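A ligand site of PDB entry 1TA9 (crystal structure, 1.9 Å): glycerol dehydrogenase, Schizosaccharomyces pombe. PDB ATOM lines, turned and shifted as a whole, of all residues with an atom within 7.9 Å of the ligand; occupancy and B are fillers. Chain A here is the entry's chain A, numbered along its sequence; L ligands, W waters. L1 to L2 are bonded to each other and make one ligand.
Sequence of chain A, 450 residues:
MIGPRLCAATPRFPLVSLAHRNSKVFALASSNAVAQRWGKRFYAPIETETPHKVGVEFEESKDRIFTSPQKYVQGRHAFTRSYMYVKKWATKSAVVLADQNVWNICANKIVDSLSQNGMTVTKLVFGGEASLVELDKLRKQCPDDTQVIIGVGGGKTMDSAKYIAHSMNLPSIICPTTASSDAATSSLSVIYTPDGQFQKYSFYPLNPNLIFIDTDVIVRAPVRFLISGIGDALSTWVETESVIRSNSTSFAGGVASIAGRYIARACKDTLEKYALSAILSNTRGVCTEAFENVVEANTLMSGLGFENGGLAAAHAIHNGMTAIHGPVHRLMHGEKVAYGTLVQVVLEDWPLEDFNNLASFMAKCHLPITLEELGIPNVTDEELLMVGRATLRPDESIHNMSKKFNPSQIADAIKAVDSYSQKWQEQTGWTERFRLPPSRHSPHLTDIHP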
ATOM      1  N   GLU A 129       5.201  -9.386  30.256  1.00  0.00           N
ATOM      2  CA  GLU A 129       4.916  -9.615  28.851  1.00  0.00           C
ATOM      3  C   GLU A 129       3.423  -9.436  28.570  1.00  0.00           C
ATOM      4  O   GLU A 129       2.602 -10.241  29.014  1.00  0.00           O
ATOM      5  CB  GLU A 129       5.361 -11.017  28.448  1.00  0.00           C
ATOM      6  N   ALA A 130       3.096  -8.388  27.829  1.00  0.00           N
ATOM      7  CA  ALA A 130       1.705  -8.103  27.487  1.00  0.00           C
ATOM      8  C   ALA A 130       1.239  -8.964  26.316  1.00  0.00           C
ATOM      9  O   ALA A 130       0.955  -8.456  25.236  1.00  0.00           O
ATOM     10  CB  ALA A 130       1.549  -6.627  27.145  1.00  0.00           C
ATOM     11  N   SER A 131       1.165 -10.265  26.550  1.00  0.00           N
ATOM     12  CA  SER A 131       0.718 -11.205  25.522  1.00  0.00           C
ATOM     13  C   SER A 131      -0.707 -11.630  25.846  1.00  0.00           C
ATOM     14  O   SER A 131      -1.104 -11.632  27.020  1.00  0.00           O
ATOM     15  CB  SER A 131       1.626 -12.435  25.476  1.00  0.00           C
ATOM     16  OG  SER A 131       1.618 -13.103  26.723  1.00  0.00           O
ATOM     17  N   LEU A 132      -1.470 -11.993  24.829  1.00  0.00           N
ATOM     18  CA  LEU A 132      -2.846 -12.405  25.023  1.00  0.00           C
ATOM     19  C   LEU A 132      -2.975 -13.561  26.014  1.00  0.00           C
ATOM     20  O   LEU A 132      -3.902 -13.602  26.818  1.00  0.00           O
ATOM     21  CB  LEU A 132      -3.478 -12.789  23.685  1.00  0.00           C
ATOM     22  CG  LEU A 132      -3.455 -11.699  22.612  1.00  0.00           C
ATOM     23  CD1 LEU A 132      -4.198 -12.170  21.367  1.00  0.00           C
ATOM     24  CD2 LEU A 132      -4.090 -10.428  23.153  1.00  0.00           C
ATOM     25  N   VAL A 133      -2.022 -14.497  25.977  1.00  0.00           N
ATOM     26  CA  VAL A 133      -2.064 -15.628  26.892  1.00  0.00           C
ATOM     27  C   VAL A 133      -1.894 -15.163  28.325  1.00  0.00           C
ATOM     28  O   VAL A 133      -2.642 -15.577  29.218  1.00  0.00           O
ATOM     29  CB  VAL A 133      -0.955 -16.660  26.563  1.00  0.00           C
ATOM     30  CG1 VAL A 133      -0.965 -17.789  27.594  1.00  0.00           C
ATOM     31  CG2 VAL A 133      -1.160 -17.221  25.172  1.00  0.00           C
ATOM     32  N   LEU A 135      -2.390 -12.144  29.485  1.00  0.00           N
ATOM     33  CA  LEU A 135      -3.487 -11.252  29.853  1.00  0.00           C
ATOM     34  C   LEU A 135      -4.714 -12.051  30.283  1.00  0.00           C
ATOM     35  O   LEU A 135      -5.416 -11.677  31.226  1.00  0.00           O
ATOM     36  CB  LEU A 135      -3.844 -10.347  28.676  1.00  0.00           C
ATOM     37  CG  LEU A 135      -2.785  -9.323  28.278  1.00  0.00           C
ATOM     38  CD1 LEU A 135      -3.154  -8.667  26.950  1.00  0.00           C
ATOM     39  CD2 LEU A 135      -2.661  -8.274  29.361  1.00  0.00           C
ATOM     40  N   GLY A 155       4.417   1.362  30.033  1.00  0.00           N
ATOM     41  CA  GLY A 155       3.516   1.072  28.932  1.00  0.00           C
ATOM     42  C   GLY A 155       2.906  -0.315  28.818  1.00  0.00           C
ATOM     43  O   GLY A 155       1.732  -0.448  28.497  1.00  0.00           O
ATOM     44  N   LYS A 156       3.694  -1.360  29.054  1.00  0.00           N
ATOM     45  CA  LYS A 156       3.168  -2.710  28.959  1.00  0.00           C
ATOM     46  C   LYS A 156       2.138  -2.981  30.050  1.00  0.00           C
ATOM     47  O   LYS A 156       1.124  -3.644  29.803  1.00  0.00           O
ATOM     48  CB  LYS A 156       4.303  -3.749  29.047  1.00  0.00           C
ATOM     49  CG  LYS A 156       5.189  -3.781  27.812  1.00  0.00           C
ATOM     50  CD  LYS A 156       6.335  -4.765  27.973  1.00  0.00           C
ATOM     51  CE  LYS A 156       7.259  -4.732  26.769  1.00  0.00           C
ATOM     52  NZ  LYS A 156       8.452  -5.617  26.945  1.00  0.00           N
ATOM     53  N   ASP A 159      -1.012  -0.848  29.140  1.00  0.00           N
ATOM     54  CA  ASP A 159      -1.768  -1.454  28.052  1.00  0.00           C
ATOM     55  C   ASP A 159      -2.457  -2.738  28.506  1.00  0.00           C
ATOM     56  O   ASP A 159      -3.534  -3.067  28.031  1.00  0.00           O
ATOM     57  CB  ASP A 159      -0.852  -1.747  26.857  1.00  0.00           C
ATOM     58  CG  ASP A 159      -0.551  -0.511  26.041  1.00  0.00           C
ATOM     59  OD1 ASP A 159      -1.475   0.291  25.808  1.00  0.00           O
ATOM     60  OD2 ASP A 159       0.609  -0.336  25.618  1.00  0.00           O
ATOM     61  N   SER A 160      -1.820  -3.455  29.432  1.00  0.00           N
ATOM     62  CA  SER A 160      -2.407  -4.689  29.953  1.00  0.00           C
ATOM     63  C   SER A 160      -3.662  -4.358  30.760  1.00  0.00           C
ATOM     64  O   SER A 160      -4.684  -5.043  30.655  1.00  0.00           O
ATOM     65  CB  SER A 160      -1.400  -5.438  30.838  1.00  0.00           C
ATOM     66  OG  SER A 160      -0.307  -5.910  30.071  1.00  0.00           O
ATOM     67  N   TYR A 163      -6.496  -3.441  28.433  1.00  0.00           N
ATOM     68  CA  TYR A 163      -7.001  -4.643  27.775  1.00  0.00           C
ATOM     69  C   TYR A 163      -7.929  -5.444  28.692  1.00  0.00           C
ATOM     70  O   TYR A 163      -9.022  -5.840  28.288  1.00  0.00           O
ATOM     71  CB  TYR A 163      -5.847  -5.544  27.339  1.00  0.00           C
ATOM     72  CG  TYR A 163      -6.285  -6.757  26.563  1.00  0.00           C
ATOM     73  CD1 TYR A 163      -6.482  -6.685  25.191  1.00  0.00           C
ATOM     74  CD2 TYR A 163      -6.547  -7.968  27.214  1.00  0.00           C
ATOM     75  CE1 TYR A 163      -6.926  -7.796  24.467  1.00  0.00           C
ATOM     76  CE2 TYR A 163      -6.994  -9.080  26.501  1.00  0.00           C
ATOM     77  CZ  TYR A 163      -7.176  -8.980  25.126  1.00  0.00           C
ATOM     78  OH  TYR A 163      -7.606 -10.080  24.419  1.00  0.00           O
ATOM     79  N   SER A 189      -3.696   1.151  21.639  1.00  0.00           N
ATOM     80  CA  SER A 189      -2.602   0.322  22.119  1.00  0.00           C
ATOM     81  C   SER A 189      -1.828  -0.187  20.917  1.00  0.00           C
ATOM     82  O   SER A 189      -2.398  -0.776  20.002  1.00  0.00           O
ATOM     83  CB  SER A 189      -3.133  -0.846  22.938  1.00  0.00           C
ATOM     84  OG  SER A 189      -3.630  -0.405  24.181  1.00  0.00           O
ATOM     85  N   VAL A 190      -0.525   0.060  20.923  1.00  0.00           N
ATOM     86  CA  VAL A 190       0.334  -0.391  19.827  1.00  0.00           C
ATOM     87  C   VAL A 190       0.327  -1.910  19.790  1.00  0.00           C
ATOM     88  O   VAL A 190       0.478  -2.569  20.812  1.00  0.00           O
ATOM     89  CB  VAL A 190       1.757   0.135  20.030  1.00  0.00           C
ATOM     90  N   ILE A 191       0.133  -2.456  18.582  1.00  0.00           N
ATOM     91  CA  ILE A 191       0.121  -3.897  18.385  1.00  0.00           C
ATOM     92  C   ILE A 191       1.386  -4.293  17.637  1.00  0.00           C
ATOM     93  O   ILE A 191       1.620  -3.848  16.512  1.00  0.00           O
ATOM     94  CB  ILE A 191      -1.104  -4.339  17.559  1.00  0.00           C
ATOM     95  CG1 ILE A 191      -2.394  -3.867  18.236  1.00  0.00           C
ATOM     96  CG2 ILE A 191      -1.109  -5.846  17.387  1.00  0.00           C
ATOM     97  CD1 ILE A 191      -2.591  -4.433  19.629  1.00  0.00           C
ATOM     98  N   TYR A 192       2.217  -5.115  18.281  1.00  0.00           N
ATOM     99  CA  TYR A 192       3.467  -5.565  17.679  1.00  0.00           C
ATOM    100  C   TYR A 192       3.587  -7.085  17.732  1.00  0.00           C
ATOM    101  O   TYR A 192       4.176  -7.704  16.840  1.00  0.00           O
ATOM    102  CB  TYR A 192       4.651  -4.918  18.394  1.00  0.00           C
ATOM    103  N   GLN A 197       8.189  -5.475  16.068  1.00  0.00           N
ATOM    104  CA  GLN A 197       7.848  -4.767  14.839  1.00  0.00           C
ATOM    105  C   GLN A 197       6.397  -4.271  14.873  1.00  0.00           C
ATOM    106  O   GLN A 197       5.471  -5.064  15.057  1.00  0.00           O
ATOM    107  CB  GLN A 197       8.055  -5.673  13.630  1.00  0.00           C
ATOM    108  N   GLN A 199       2.757  -3.204  13.841  1.00  0.00           N
ATOM    109  CA  GLN A 199       1.848  -3.754  12.842  1.00  0.00           C
ATOM    110  C   GLN A 199       0.697  -2.785  12.573  1.00  0.00           C
ATOM    111  O   GLN A 199       0.437  -2.417  11.430  1.00  0.00           O
ATOM    112  CB  GLN A 199       1.306  -5.099  13.321  1.00  0.00           C
ATOM    113  N   LYS A 200       0.012  -2.369  13.632  1.00  0.00           N
ATOM    114  CA  LYS A 200      -1.107  -1.451  13.502  1.00  0.00           C
ATOM    115  C   LYS A 200      -1.527  -0.879  14.848  1.00  0.00           C
ATOM    116  O   LYS A 200      -1.006  -1.272  15.897  1.00  0.00           O
ATOM    117  CB  LYS A 200      -2.293  -2.145  12.844  1.00  0.00           C
ATOM    118  N   SER A 202      -4.580  -0.241  17.631  1.00  0.00           N
ATOM    119  CA  SER A 202      -5.868  -0.770  18.077  1.00  0.00           C
ATOM    120  C   SER A 202      -6.593   0.336  18.844  1.00  0.00           C
ATOM    121  O   SER A 202      -6.033   0.914  19.775  1.00  0.00           O
ATOM    122  CB  SER A 202      -5.651  -1.981  18.985  1.00  0.00           C
ATOM    123  N   TYR A 204      -9.627   1.454  21.305  1.00  0.00           N
ATOM    124  CA  TYR A 204     -10.693   1.084  22.235  1.00  0.00           C
ATOM    125  C   TYR A 204     -11.807   2.110  22.027  1.00  0.00           C
ATOM    126  O   TYR A 204     -11.542   3.249  21.650  1.00  0.00           O
ATOM    127  CB  TYR A 204     -10.186   1.158  23.676  1.00  0.00           C
ATOM    128  CG  TYR A 204      -9.259   0.016  24.045  1.00  0.00           C
ATOM    129  CD1 TYR A 204      -9.740  -1.284  24.159  1.00  0.00           C
ATOM    130  CD2 TYR A 204      -7.903   0.233  24.252  1.00  0.00           C
ATOM    131  CE1 TYR A 204      -8.887  -2.346  24.475  1.00  0.00           C
ATOM    132  CE2 TYR A 204      -7.039  -0.810  24.564  1.00  0.00           C
ATOM    133  CZ  TYR A 204      -7.537  -2.101  24.673  1.00  0.00           C
ATOM    134  OH  TYR A 204      -6.690  -3.149  24.948  1.00  0.00           O
HETATM  135  N1  LIG L   1       0.386  -4.358  22.879  1.00  0.00           N
HETATM  136  C1  LIG L   1       0.081  -5.817  22.824  1.00  0.00           C
HETATM  137  C2  LIG L   1       1.062  -6.552  21.918  1.00  0.00           C
HETATM  138  O1  LIG L   1       1.320  -6.127  20.787  1.00  0.00           O
HETATM  139  C3  LIG L   1      -1.341  -6.044  22.334  1.00  0.00           C
HETATM  140  N1  LG2 L   2       1.608  -7.659  22.421  1.00  0.00           N
HETATM  141  C1  LG2 L   2       2.547  -8.472  21.671  1.00  0.00           C
HETATM  142  C2  LG2 L   2       1.815  -9.643  21.023  1.00  0.00           C
HETATM  143  O1  LG2 L   2       1.648 -10.671  21.715  1.00  0.00           O
HETATM  144  C3  LG2 L   2       3.642  -8.988  22.590  1.00  0.00           C
HETATM  145  O2  LG2 L   2       1.406  -9.515  19.848  1.00  0.00           O
HETATM  146  O   HOH W   1      -2.212  -5.003  24.783  1.00  0.00           O
HETATM  147  O   HOH W   2      -0.514 -12.510  22.126  1.00  0.00           O
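Ser 131 touches the ligand. CD1 of Ile 191 touches C3 of LIG L1, 3.4 Å away. Hydrophobic or aromatic side chains that line the ligand: Ile 191. Within 4 Å of the ligand: Ala 130, Ser 131, Val 190, Ile 191 and Tyr 192.
The backbone NH of Ile 191 lies within hydrogen-bond range of the backbone carbonyl oxygen of Lys 200 (3.1 Å). O of Ile 191 sits at hydrogen-bond distance from N of Gln 199, 3.0 Å away.
N1 of LIG L1 sits at hydrogen-bond distance from O of Val 190 (2.7 Å). An oxygen (O1) of LIG L1 sits at hydrogen-bond distance from the backbone NH of Tyr 192, at 2.8 Å. A nitrogen (N1) of LG2 L2 lies within hydrogen-bond range of the backbone carbonyl oxygen of Ala 130 (3.0 Å).
Water W2 bridges an oxygen (O1) of LG2 L2 (2.9 Å) and the backbone NH (N) of Leu 132 (2.9 Å).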
